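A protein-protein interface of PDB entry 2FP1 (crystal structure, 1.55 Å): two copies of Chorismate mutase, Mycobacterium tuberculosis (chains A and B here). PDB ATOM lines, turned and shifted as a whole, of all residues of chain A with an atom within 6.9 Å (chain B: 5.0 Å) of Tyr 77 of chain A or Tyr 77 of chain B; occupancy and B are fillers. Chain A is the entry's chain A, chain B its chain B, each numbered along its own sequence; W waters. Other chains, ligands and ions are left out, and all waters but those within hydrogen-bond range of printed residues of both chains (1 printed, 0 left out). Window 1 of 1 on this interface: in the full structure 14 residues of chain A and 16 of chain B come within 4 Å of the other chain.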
ATOM      1  N   ALA A  24     -20.142  29.417  13.258  1.00  0.00           N
ATOM      2  CA  ALA A  24     -19.402  28.173  13.113  1.00  0.00           C
ATOM      3  C   ALA A  24     -20.273  27.091  12.481  1.00  0.00           C
ATOM      4  O   ALA A  24     -19.805  26.372  11.603  1.00  0.00           O
ATOM      5  CB  ALA A  24     -18.853  27.707  14.497  1.00  0.00           C
ATOM      6  N   TRP A  28     -19.295  25.245   9.092  1.00  0.00           N
ATOM      7  CA  TRP A  28     -19.078  23.799   9.127  1.00  0.00           C
ATOM      8  C   TRP A  28     -19.839  23.158   7.970  1.00  0.00           C
ATOM      9  O   TRP A  28     -19.256  22.386   7.241  1.00  0.00           O
ATOM     10  CB  TRP A  28     -19.484  23.215  10.470  1.00  0.00           C
ATOM     11  CG  TRP A  28     -19.327  21.706  10.552  1.00  0.00           C
ATOM     12  CD1 TRP A  28     -20.295  20.796  10.333  1.00  0.00           C
ATOM     13  CD2 TRP A  28     -18.142  20.981  10.838  1.00  0.00           C
ATOM     14  NE1 TRP A  28     -19.798  19.524  10.479  1.00  0.00           N
ATOM     15  CE2 TRP A  28     -18.475  19.610  10.812  1.00  0.00           C
ATOM     16  CE3 TRP A  28     -16.850  21.353  11.190  1.00  0.00           C
ATOM     17  CZ2 TRP A  28     -17.552  18.619  11.092  1.00  0.00           C
ATOM     18  CZ3 TRP A  28     -15.937  20.377  11.480  1.00  0.00           C
ATOM     19  CH2 TRP A  28     -16.284  19.009  11.384  1.00  0.00           C
ATOM     20  N   LEU A  32     -16.420  26.052   4.943  1.00  0.00           N
ATOM     21  CA  LEU A  32     -15.614  27.273   4.865  1.00  0.00           C
ATOM     22  C   LEU A  32     -14.648  27.295   6.034  1.00  0.00           C
ATOM     23  O   LEU A  32     -14.944  26.728   7.072  1.00  0.00           O
ATOM     24  CB  LEU A  32     -16.495  28.509   4.945  1.00  0.00           C
ATOM     25  CG  LEU A  32     -17.560  28.615   3.847  1.00  0.00           C
ATOM     26  CD1 LEU A  32     -18.415  29.802   4.105  1.00  0.00           C
ATOM     27  CD2 LEU A  32     -16.875  28.702   2.491  1.00  0.00           C
ATOM     28  N   PRO A  33     -13.485  27.915   5.852  1.00  0.00           N
ATOM     29  CA  PRO A  33     -12.603  28.005   7.004  1.00  0.00           C
ATOM     30  C   PRO A  33     -13.092  29.037   7.971  1.00  0.00           C
ATOM     31  O   PRO A  33     -13.904  29.906   7.651  1.00  0.00           O
ATOM     32  CB  PRO A  33     -11.289  28.445   6.402  1.00  0.00           C
ATOM     33  CG  PRO A  33     -11.676  29.165   5.162  1.00  0.00           C
ATOM     34  CD  PRO A  33     -12.917  28.575   4.664  1.00  0.00           C
ATOM     35  N   ILE A  34     -12.604  28.948   9.189  1.00  0.00           N
ATOM     36  CA  ILE A  34     -12.899  29.938  10.218  1.00  0.00           C
ATOM     37  C   ILE A  34     -12.272  31.286   9.903  1.00  0.00           C
ATOM     38  O   ILE A  34     -12.921  32.335   9.988  1.00  0.00           O
ATOM     39  CB  ILE A  34     -12.349  29.465  11.617  1.00  0.00           C
ATOM     40  CG1 ILE A  34     -13.014  28.155  12.082  1.00  0.00           C
ATOM     41  CG2 ILE A  34     -12.480  30.581  12.670  1.00  0.00           C
ATOM     42  CD1 ILE A  34     -14.537  28.106  11.872  1.00  0.00           C
ATOM     43  N   GLU A  35     -10.987  31.251   9.586  1.00  0.00           N
ATOM     44  CA  GLU A  35     -10.168  32.461   9.463  1.00  0.00           C
ATOM     45  C   GLU A  35     -10.252  33.059   8.080  1.00  0.00           C
ATOM     46  O   GLU A  35     -10.500  32.354   7.095  1.00  0.00           O
ATOM     47  CB  GLU A  35      -8.716  32.077   9.791  1.00  0.00           C
ATOM     48  CG  GLU A  35      -7.996  31.151   8.736  1.00  0.00           C
ATOM     49  CD  GLU A  35      -8.330  29.626   8.780  1.00  0.00           C
ATOM     50  OE1 GLU A  35      -9.235  29.178   9.517  1.00  0.00           O
ATOM     51  OE2 GLU A  35      -7.673  28.875   8.011  1.00  0.00           O
ATOM     52  N   ASP A  36     -10.090  34.379   8.038  1.00  0.00           N
ATOM     53  CA  ASP A  36      -9.903  35.136   6.793  1.00  0.00           C
ATOM     54  C   ASP A  36      -9.287  36.488   7.159  1.00  0.00           C
ATOM     55  O   ASP A  36      -9.993  37.422   7.545  1.00  0.00           O
ATOM     56  CB  ASP A  36     -11.208  35.309   6.011  1.00  0.00           C
ATOM     57  CG  ASP A  36     -10.990  35.896   4.645  1.00  0.00           C
ATOM     58  OD1 ASP A  36     -10.159  36.812   4.503  1.00  0.00           O
ATOM     59  OD2 ASP A  36     -11.675  35.436   3.687  1.00  0.00           O
ATOM     60  N   ARG A  70     -10.503  37.681  17.642  1.00  0.00           N
ATOM     61  CA  ARG A  70      -9.684  36.493  17.927  1.00  0.00           C
ATOM     62  C   ARG A  70     -10.407  35.562  18.873  1.00  0.00           C
ATOM     63  O   ARG A  70     -10.434  34.330  18.662  1.00  0.00           O
ATOM     64  CB  ARG A  70      -8.330  36.868  18.531  1.00  0.00           C
ATOM     65  CG  ARG A  70      -7.370  37.403  17.496  1.00  0.00           C
ATOM     66  CD  ARG A  70      -6.067  37.884  18.118  1.00  0.00           C
ATOM     67  NE  ARG A  70      -5.659  37.070  19.268  1.00  0.00           N
ATOM     68  CZ  ARG A  70      -5.606  37.468  20.536  1.00  0.00           C
ATOM     69  NH1 ARG A  70      -5.913  38.713  20.885  1.00  0.00           N
ATOM     70  NH2 ARG A  70      -5.215  36.601  21.466  1.00  0.00           N
ATOM     71  N   THR A  72     -13.543  35.240  19.268  1.00  0.00           N
ATOM     72  CA  THR A  72     -14.673  34.677  18.561  1.00  0.00           C
ATOM     73  C   THR A  72     -14.212  33.532  17.705  1.00  0.00           C
ATOM     74  O   THR A  72     -14.813  32.410  17.690  1.00  0.00           O
ATOM     75  CB  THR A  72     -15.340  35.786  17.715  1.00  0.00           C
ATOM     76  OG1 THR A  72     -15.741  36.865  18.586  1.00  0.00           O
ATOM     77  CG2 THR A  72     -16.636  35.243  17.100  1.00  0.00           C
ATOM     78  N   GLU A  73     -13.110  33.745  17.013  1.00  0.00           N
ATOM     79  CA  GLU A  73     -12.483  32.665  16.206  1.00  0.00           C
ATOM     80  C   GLU A  73     -12.124  31.460  17.062  1.00  0.00           C
ATOM     81  O   GLU A  73     -12.283  30.305  16.653  1.00  0.00           O
ATOM     82  CB  GLU A  73     -11.309  33.193  15.437  1.00  0.00           C
ATOM     83  CG  GLU A  73     -11.734  34.163  14.325  1.00  0.00           C
ATOM     84  CD  GLU A  73     -10.605  34.940  13.689  1.00  0.00           C
ATOM     85  OE1 GLU A  73      -9.578  35.186  14.339  1.00  0.00           O
ATOM     86  OE2 GLU A  73     -10.738  35.300  12.499  1.00  0.00           O
ATOM     87  N   ALA A  74     -11.627  31.737  18.263  1.00  0.00           N
ATOM     88  CA  ALA A  74     -11.264  30.667  19.192  1.00  0.00           C
ATOM     89  C   ALA A  74     -12.461  29.798  19.508  1.00  0.00           C
ATOM     90  O   ALA A  74     -12.329  28.571  19.576  1.00  0.00           O
ATOM     91  CB  ALA A  74     -10.757  31.280  20.517  1.00  0.00           C
ATOM     92  N   ILE A  75     -13.630  30.393  19.708  1.00  0.00           N
ATOM     93  CA  ILE A  75     -14.848  29.608  19.972  1.00  0.00           C
ATOM     94  C   ILE A  75     -15.210  28.788  18.724  1.00  0.00           C
ATOM     95  O   ILE A  75     -15.557  27.584  18.807  1.00  0.00           O
ATOM     96  CB  ILE A  75     -16.005  30.506  20.394  1.00  0.00           C
ATOM     97  CG1 ILE A  75     -15.744  31.141  21.769  1.00  0.00           C
ATOM     98  CG2 ILE A  75     -17.329  29.717  20.487  1.00  0.00           C
ATOM     99  CD1 ILE A  75     -16.678  32.370  22.100  1.00  0.00           C
ATOM    100  N   GLU A  76     -15.094  29.395  17.560  1.00  0.00           N
ATOM    101  CA  GLU A  76     -15.439  28.713  16.323  1.00  0.00           C
ATOM    102  C   GLU A  76     -14.522  27.497  16.159  1.00  0.00           C
ATOM    103  O   GLU A  76     -14.988  26.410  15.822  1.00  0.00           O
ATOM    104  CB  GLU A  76     -15.356  29.659  15.108  1.00  0.00           C
ATOM    105  CG  GLU A  76     -16.346  30.804  15.175  1.00  0.00           C
ATOM    106  CD  GLU A  76     -16.222  31.759  14.044  1.00  0.00           C
ATOM    107  OE1 GLU A  76     -16.193  31.320  12.906  1.00  0.00           O
ATOM    108  OE2 GLU A  76     -16.081  33.005  14.305  1.00  0.00           O
ATOM    109  N   TYR A  77     -13.236  27.662  16.377  1.00  0.00           N
ATOM    110  CA  TYR A  77     -12.330  26.521  16.271  1.00  0.00           C
ATOM    111  C   TYR A  77     -12.678  25.419  17.281  1.00  0.00           C
ATOM    112  O   TYR A  77     -12.574  24.229  16.983  1.00  0.00           O
ATOM    113  CB  TYR A  77     -10.887  26.962  16.519  1.00  0.00           C
ATOM    114  CG  TYR A  77     -10.202  27.614  15.320  1.00  0.00           C
ATOM    115  CD1 TYR A  77     -10.220  27.017  14.060  1.00  0.00           C
ATOM    116  CD2 TYR A  77      -9.504  28.815  15.454  1.00  0.00           C
ATOM    117  CE1 TYR A  77      -9.548  27.582  12.985  1.00  0.00           C
ATOM    118  CE2 TYR A  77      -8.829  29.355  14.406  1.00  0.00           C
ATOM    119  CZ  TYR A  77      -8.889  28.756  13.159  1.00  0.00           C
ATOM    120  OH  TYR A  77      -8.220  29.317  12.094  1.00  0.00           O
ATOM    121  N   SER A  78     -13.035  25.807  18.501  1.00  0.00           N
ATOM    122  CA  SER A  78     -13.398  24.797  19.515  1.00  0.00           C
ATOM    123  C   SER A  78     -14.604  23.969  19.044  1.00  0.00           C
ATOM    124  O   SER A  78     -14.632  22.747  19.206  1.00  0.00           O
ATOM    125  CB  SER A  78     -13.691  25.485  20.836  1.00  0.00           C
ATOM    126  OG  SER A  78     -13.927  24.515  21.848  1.00  0.00           O
ATOM    127  N   ARG A  79     -15.583  24.613  18.426  1.00  0.00           N
ATOM    128  CA  ARG A  79     -16.735  23.856  17.940  1.00  0.00           C
ATOM    129  C   ARG A  79     -16.277  22.915  16.840  1.00  0.00           C
ATOM    130  O   ARG A  79     -16.747  21.774  16.736  1.00  0.00           O
ATOM    131  CB  ARG A  79     -17.791  24.768  17.389  1.00  0.00           C
ATOM    132  CG  ARG A  79     -18.468  25.684  18.389  1.00  0.00           C
ATOM    133  CD  ARG A  79     -18.635  25.147  19.772  1.00  0.00           C
ATOM    134  NE  ARG A  79     -19.512  26.023  20.557  1.00  0.00           N
ATOM    135  CZ  ARG A  79     -19.601  26.018  21.874  1.00  0.00           C
ATOM    136  NH1 ARG A  79     -18.810  25.231  22.601  1.00  0.00           N
ATOM    137  NH2 ARG A  79     -20.503  26.775  22.470  1.00  0.00           N
ATOM    138  N   PHE A  80     -15.462  23.409  15.917  1.00  0.00           N
ATOM    139  CA  PHE A  80     -14.956  22.531  14.842  1.00  0.00           C
ATOM    140  C   PHE A  80     -14.231  21.307  15.422  1.00  0.00           C
ATOM    141  O   PHE A  80     -14.345  20.201  14.915  1.00  0.00           O
ATOM    142  CB  PHE A  80     -14.044  23.272  13.878  1.00  0.00           C
ATOM    143  CG  PHE A  80     -14.753  23.949  12.724  1.00  0.00           C
ATOM    144  CD1 PHE A  80     -15.966  24.549  12.878  1.00  0.00           C
ATOM    145  CD2 PHE A  80     -14.132  24.034  11.512  1.00  0.00           C
ATOM    146  CE1 PHE A  80     -16.601  25.198  11.800  1.00  0.00           C
ATOM    147  CE2 PHE A  80     -14.735  24.697  10.415  1.00  0.00           C
ATOM    148  CZ  PHE A  80     -15.961  25.287  10.587  1.00  0.00           C
ATOM    149  N   SER A  81     -13.502  21.497  16.495  1.00  0.00           N
ATOM    150  CA  SER A  81     -12.845  20.364  17.166  1.00  0.00           C
ATOM    151  C   SER A  81     -13.902  19.360  17.605  1.00  0.00           C
ATOM    152  O   SER A  81     -13.742  18.151  17.372  1.00  0.00           O
ATOM    153  CB  SER A  81     -11.985  20.857  18.333  1.00  0.00           C
ATOM    154  OG  SER A  81     -11.449  19.802  19.101  1.00  0.00           O
ATOM    155  N   ASP A  82     -14.925  19.846  18.309  1.00  0.00           N
ATOM    156  CA  ASP A  82     -16.029  19.029  18.823  1.00  0.00           C
ATOM    157  C   ASP A  82     -16.696  18.257  17.700  1.00  0.00           C
ATOM    158  O   ASP A  82     -17.049  17.086  17.855  1.00  0.00           O
ATOM    159  CB  ASP A  82     -17.075  19.913  19.483  1.00  0.00           C
ATOM    160  CG  ASP A  82     -16.639  20.518  20.821  1.00  0.00           C
ATOM    161  OD1 ASP A  82     -15.600  20.107  21.399  1.00  0.00           O
ATOM    162  OD2 ASP A  82     -17.390  21.432  21.308  1.00  0.00           O
ATOM    163  N   TRP A  83     -16.919  18.917  16.580  1.00  0.00           N
ATOM    164  CA  TRP A  83     -17.687  18.325  15.476  1.00  0.00           C
ATOM    165  C   TRP A  83     -16.842  17.329  14.688  1.00  0.00           C
ATOM    166  O   TRP A  83     -17.378  16.411  14.071  1.00  0.00           O
ATOM    167  CB  TRP A  83     -18.303  19.429  14.583  1.00  0.00           C
ATOM    168  CG  TRP A  83     -19.245  20.297  15.343  1.00  0.00           C
ATOM    169  CD1 TRP A  83     -19.956  19.963  16.481  1.00  0.00           C
ATOM    170  CD2 TRP A  83     -19.584  21.658  15.069  1.00  0.00           C
ATOM    171  NE1 TRP A  83     -20.687  21.027  16.928  1.00  0.00           N
ATOM    172  CE2 TRP A  83     -20.493  22.079  16.077  1.00  0.00           C
ATOM    173  CE3 TRP A  83     -19.213  22.559  14.082  1.00  0.00           C
ATOM    174  CZ2 TRP A  83     -21.029  23.364  16.124  1.00  0.00           C
ATOM    175  CZ3 TRP A  83     -19.753  23.858  14.141  1.00  0.00           C
ATOM    176  CH2 TRP A  83     -20.630  24.232  15.148  1.00  0.00           C
ATOM    177  N   LYS A  84     -15.531  17.487  14.703  1.00  0.00           N
ATOM    178  CA  LYS A  84     -14.624  16.458  14.124  1.00  0.00           C
ATOM    179  C   LYS A  84     -14.681  15.178  14.925  1.00  0.00           C
ATOM    180  O   LYS A  84     -14.658  14.080  14.367  1.00  0.00           O
ATOM    181  CB  LYS A  84     -13.169  16.894  14.065  1.00  0.00           C
ATOM    182  CG  LYS A  84     -12.853  17.753  12.887  1.00  0.00           C
ATOM    183  CD  LYS A  84     -12.749  16.935  11.602  1.00  0.00           C
ATOM    184  CE  LYS A  84     -12.312  17.827  10.449  1.00  0.00           C
ATOM    185  NZ  LYS A  84     -12.288  17.160   9.143  1.00  0.00           N
ATOM    186  N   ILE B  34      -6.190  23.899   8.220  1.00  0.00           N
ATOM    187  CA  ILE B  34      -6.189  22.592   8.863  1.00  0.00           C
ATOM    188  C   ILE B  34      -6.724  21.501   7.946  1.00  0.00           C
ATOM    189  O   ILE B  34      -6.138  20.416   7.895  1.00  0.00           O
ATOM    190  CB  ILE B  34      -6.974  22.644  10.180  1.00  0.00           C
ATOM    191  CG1 ILE B  34      -6.153  23.413  11.220  1.00  0.00           C
ATOM    192  CG2 ILE B  34      -7.311  21.213  10.712  1.00  0.00           C
ATOM    193  CD1 ILE B  34      -6.830  23.588  12.496  1.00  0.00           C
ATOM    194  N   GLU B  35      -7.806  21.788   7.219  1.00  0.00           N
ATOM    195  CA  GLU B  35      -8.402  20.804   6.322  1.00  0.00           C
ATOM    196  C   GLU B  35      -7.509  20.585   5.105  1.00  0.00           C
ATOM    197  O   GLU B  35      -6.904  21.521   4.608  1.00  0.00           O
ATOM    198  CB  GLU B  35      -9.763  21.251   5.824  1.00  0.00           C
ATOM    199  CG  GLU B  35     -10.839  21.402   6.882  1.00  0.00           C
ATOM    200  CD  GLU B  35     -11.249  20.104   7.551  1.00  0.00           C
ATOM    201  OE1 GLU B  35     -11.349  19.059   6.868  1.00  0.00           O
ATOM    202  OE2 GLU B  35     -11.561  20.149   8.759  1.00  0.00           O
ATOM    203  N   GLU B  73      -7.246  15.844  13.452  1.00  0.00           N
ATOM    204  CA  GLU B  73      -7.773  17.156  12.987  1.00  0.00           C
ATOM    205  C   GLU B  73      -8.467  17.855  14.180  1.00  0.00           C
ATOM    206  O   GLU B  73      -8.350  19.077  14.390  1.00  0.00           O
ATOM    207  CB  GLU B  73      -8.717  17.013  11.806  1.00  0.00           C
ATOM    208  CG  GLU B  73      -7.993  16.573  10.551  1.00  0.00           C
ATOM    209  CD  GLU B  73      -8.900  16.224   9.391  1.00  0.00           C
ATOM    210  OE1 GLU B  73     -10.021  15.746   9.615  1.00  0.00           O
ATOM    211  OE2 GLU B  73      -8.425  16.384   8.239  1.00  0.00           O
ATOM    212  N   ALA B  74      -9.166  17.077  14.995  1.00  0.00           N
ATOM    213  CA  ALA B  74      -9.857  17.666  16.148  1.00  0.00           C
ATOM    214  C   ALA B  74      -8.877  18.310  17.130  1.00  0.00           C
ATOM    215  O   ALA B  74      -9.138  19.371  17.712  1.00  0.00           O
ATOM    216  CB  ALA B  74     -10.691  16.582  16.881  1.00  0.00           C
ATOM    217  N   ILE B  75      -7.724  17.670  17.315  1.00  0.00           N
ATOM    218  CA  ILE B  75      -6.709  18.185  18.211  1.00  0.00           C
ATOM    219  C   ILE B  75      -6.118  19.468  17.613  1.00  0.00           C
ATOM    220  O   ILE B  75      -5.963  20.459  18.320  1.00  0.00           O
ATOM    221  CB  ILE B  75      -5.630  17.164  18.459  1.00  0.00           C
ATOM    222  CG1 ILE B  75      -6.189  16.051  19.367  1.00  0.00           C
ATOM    223  CG2 ILE B  75      -4.423  17.838  19.129  1.00  0.00           C
ATOM    224  CD1 ILE B  75      -5.331  14.776  19.297  1.00  0.00           C
ATOM    225  N   GLU B  76      -5.811  19.432  16.320  1.00  0.00           N
ATOM    226  CA  GLU B  76      -5.300  20.652  15.658  1.00  0.00           C
ATOM    227  C   GLU B  76      -6.270  21.848  15.873  1.00  0.00           C
ATOM    228  O   GLU B  76      -5.863  22.982  16.215  1.00  0.00           O
ATOM    229  CB  GLU B  76      -5.115  20.407  14.173  1.00  0.00           C
ATOM    230  CG  GLU B  76      -4.134  19.330  13.802  1.00  0.00           C
ATOM    231  CD  GLU B  76      -4.086  19.131  12.302  1.00  0.00           C
ATOM    232  OE1 GLU B  76      -3.603  20.027  11.582  1.00  0.00           O
ATOM    233  OE2 GLU B  76      -4.581  18.086  11.819  1.00  0.00           O
ATOM    234  N   TYR B  77      -7.562  21.627  15.639  1.00  0.00           N
ATOM    235  CA  TYR B  77      -8.555  22.713  15.846  1.00  0.00           C
ATOM    236  C   TYR B  77      -8.570  23.184  17.293  1.00  0.00           C
ATOM    237  O   TYR B  77      -8.696  24.381  17.556  1.00  0.00           O
ATOM    238  CB  TYR B  77      -9.949  22.250  15.461  1.00  0.00           C
ATOM    239  CG  TYR B  77     -10.243  22.254  13.970  1.00  0.00           C
ATOM    240  CD1 TYR B  77     -10.070  23.401  13.234  1.00  0.00           C
ATOM    241  CD2 TYR B  77     -10.717  21.137  13.327  1.00  0.00           C
ATOM    242  CE1 TYR B  77     -10.350  23.436  11.906  1.00  0.00           C
ATOM    243  CE2 TYR B  77     -11.015  21.164  11.968  1.00  0.00           C
ATOM    244  CZ  TYR B  77     -10.809  22.313  11.266  1.00  0.00           C
ATOM    245  OH  TYR B  77     -11.088  22.379   9.907  1.00  0.00           O
ATOM    246  N   SER B  78      -8.422  22.270  18.236  1.00  0.00           N
ATOM    247  CA  SER B  78      -8.432  22.657  19.633  1.00  0.00           C
ATOM    248  C   SER B  78      -7.223  23.537  19.977  1.00  0.00           C
ATOM    249  O   SER B  78      -7.335  24.492  20.735  1.00  0.00           O
ATOM    250  CB  SER B  78      -8.502  21.392  20.537  1.00  0.00           C
ATOM    251  OG  SER B  78      -8.584  21.740  21.916  1.00  0.00           O
ATOM    252  N   ARG B  79      -6.062  23.160  19.456  1.00  0.00           N
ATOM    253  CA  ARG B  79      -4.875  23.966  19.644  1.00  0.00           C
ATOM    254  C   ARG B  79      -5.019  25.316  18.998  1.00  0.00           C
ATOM    255  O   ARG B  79      -4.688  26.317  19.620  1.00  0.00           O
ATOM    256  CB  ARG B  79      -3.627  23.254  19.136  1.00  0.00           C
ATOM    257  CG  ARG B  79      -3.308  21.998  19.911  1.00  0.00           C
ATOM    258  CD  ARG B  79      -3.086  22.213  21.366  1.00  0.00           C
ATOM    259  NE  ARG B  79      -2.241  21.126  21.862  1.00  0.00           N
ATOM    260  CZ  ARG B  79      -2.612  20.223  22.763  1.00  0.00           C
ATOM    261  NH1 ARG B  79      -3.799  20.288  23.344  1.00  0.00           N
ATOM    262  NH2 ARG B  79      -1.749  19.274  23.129  1.00  0.00           N
ATOM    263  N   PHE B  80      -5.556  25.376  17.786  1.00  0.00           N
ATOM    264  CA  PHE B  80      -5.805  26.717  17.177  1.00  0.00           C
ATOM    265  C   PHE B  80      -6.721  27.544  18.053  1.00  0.00           C
ATOM    266  O   PHE B  80      -6.526  28.757  18.186  1.00  0.00           O
ATOM    267  CB  PHE B  80      -6.412  26.624  15.796  1.00  0.00           C
ATOM    268  CG  PHE B  80      -5.411  26.496  14.685  1.00  0.00           C
ATOM    269  CD1 PHE B  80      -4.268  25.730  14.836  1.00  0.00           C
ATOM    270  CD2 PHE B  80      -5.621  27.149  13.486  1.00  0.00           C
ATOM    271  CE1 PHE B  80      -3.376  25.616  13.814  1.00  0.00           C
ATOM    272  CE2 PHE B  80      -4.693  27.029  12.435  1.00  0.00           C
ATOM    273  CZ  PHE B  80      -3.564  26.273  12.619  1.00  0.00           C
ATOM    274  N   SER B  81      -7.721  26.915  18.676  1.00  0.00           N
ATOM    275  CA  SER B  81      -8.583  27.645  19.602  1.00  0.00           C
ATOM    276  C   SER B  81      -7.779  28.215  20.774  1.00  0.00           C
ATOM    277  O   SER B  81      -7.860  29.395  21.090  1.00  0.00           O
ATOM    278  CB  SER B  81      -9.677  26.728  20.131  1.00  0.00           C
ATOM    279  OG  SER B  81     -10.473  27.359  21.124  1.00  0.00           O
ATOM    280  N   LYS B  84      -5.583  31.088  19.596  1.00  0.00           N
ATOM    281  CA  LYS B  84      -6.332  32.331  19.375  1.00  0.00           C
ATOM    282  C   LYS B  84      -6.593  33.040  20.686  1.00  0.00           C
ATOM    283  O   LYS B  84      -6.676  34.294  20.700  1.00  0.00           O
ATOM    284  CB  LYS B  84      -7.641  32.061  18.656  1.00  0.00           C
ATOM    285  CG  LYS B  84      -7.532  31.828  17.158  1.00  0.00           C
ATOM    286  CD  LYS B  84      -7.279  33.147  16.408  1.00  0.00           C
ATOM    287  CE  LYS B  84      -7.073  32.947  14.909  1.00  0.00           C
ATOM    288  NZ  LYS B  84      -6.835  34.312  14.282  1.00  0.00           N
HETATM  289  O   HOH W   1      -8.131  26.143   8.915  1.00  0.00           O
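OG of Ser 81 of chain B sits at hydrogen-bond distance from O of Ala 74 of chain A, at 2.7 Å. The side-chain carboxylate (OE1) of Glu 73 of chain B is in salt-bridge range of the side-chain amino group (NZ) of Lys 84 of chain A (2.7 Å). The side-chain amino group of Lys 84 of chain A is in salt-bridge range of the side-chain carboxylate of Glu 35 of chain B, at 3.1 Å. The guanidinium group (NH2) of Arg 70 of chain A sits at hydrogen-bond distance from the backbone carbonyl oxygen (O) of Lys 84 of chain B. The side-chain carboxylate of Glu 73 of chain A is in salt-bridge range of the side-chain amino group of Lys 84 of chain B (2.9 Å). OG of Ser 81 of chain A sits at hydrogen-bond distance from O of Ala 74 of chain B (2.7 Å).
The side-chain hydroxyl of Tyr 77 of chain A sits at hydrogen-bond distance from the side-chain carboxylate of Glu 35 of chain A (2.8 Å). The side-chain carboxylate (OE2) of Glu 35 of chain B lies within hydrogen-bond range of the side-chain hydroxyl (OH) of Tyr 77 of chain B.
Among the printed residues, merely in contact across the chains: Ala 74 of chain A with Lys 84 of chain B, Tyr 77 of chain A with Tyr 77 of chain B, Tyr 77 of chain A with Phe 80 of chain B, Tyr 77 of chain A with Ser 81 of chain B, Tyr 77 of chain A with Lys 84 of chain B, Ser 78 of chain A with Ser 81 of chain B, Phe 80 of chain A with Tyr 77 of chain B, Ser 81 of chain A with Tyr 77 of chain B, Ser 81 of chain A with Ser 78 of chain B, Lys 84 of chain A with Ala 74 of chain B and Lys 84 of chain A with Tyr 77 of chain B.
Of chain B, only Tyr 77 (3.5 Å), Phe 80 (3.7 Å), Ser 81 (3.8 Å) and Lys 84 (3.9 Å) come within 4 Å of Tyr 77 of chain A. Tyr 77 of chain B touches just these residues of chain A: Tyr 77 (3.5 Å), Phe 80 (3.8 Å), Ser 81 (3.8 Å) and Lys 84 (3.9 Å). Of the printed residues of chain B, Phe 80 of chain A touches Tyr 77 (3.8 Å). Printed residues of chain B within 4 Å of Ser 81 of chain A: Ala 74 (2.7 Å), Tyr 77 (3.8 Å) and Ser 78 (3.6 Å). Of the printed residues of chain B, Ala 74 of chain A touches Ser 81 (2.7 Å) and Lys 84 (3.7 Å). Of the printed residues of chain B, Glu 73 of chain A touches Lys 84 (2.9 Å). The nearest residue of chain B that does not touch Tyr 77 of chain A is Ser 78 of chain B (4.8 Å). The nearest residue of chain A that does not touch Tyr 77 of chain B is Ser 78 of chain A (4.7 Å).
Printed residues of chain A that touch a printed residue of chain B: Arg 70, Glu 73, Ala 74, Tyr 77, Ser 78, Phe 80, Ser 81 and Lys 84. Hydrophobic or aromatic side chains of chain A that line the printed part of chain B: Ala 74, Tyr 77 and Phe 80. Of the 12 printed residues of chain B, 8 touch a printed residue of chain A. Hydrophobic or aromatic side chains of chain B that line the printed part of chain A: Ala 74, Tyr 77 and Phe 80. Among the printed residues, 17 pairs touch across the chains.
Ala 74 of chain A touches Lys 84 of chain B, and with the chains exchanged Lys 84 of chain A touches Ala 74 of chain B. Tyr 77 of chain A touches Ser 81 of chain B, and with the chains exchanged Ser 81 of chain A touches Tyr 77 of chain B. Ser 78 of chain A touches Ser 81 of chain B, and with the chains exchanged Ser 81 of chain A touches Ser 78 of chain B. Lys 84 of chain A touches Glu 35 of chain B, but with the chains exchanged Glu 35 of chain A does not touch Lys 84 of chain B (5.4 Å). 12 positions are printed for both chains. Of the 17 pairs that touch across the chains among the printed residues, 15 have their exchanged pair printed and touching as well.
Water W1 lies within hydrogen-bond range of the side-chain carboxylate of Glu 35 of chain A (2.9 Å) and the backbone NH of Ile 34 of chain B (3.0 Å).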
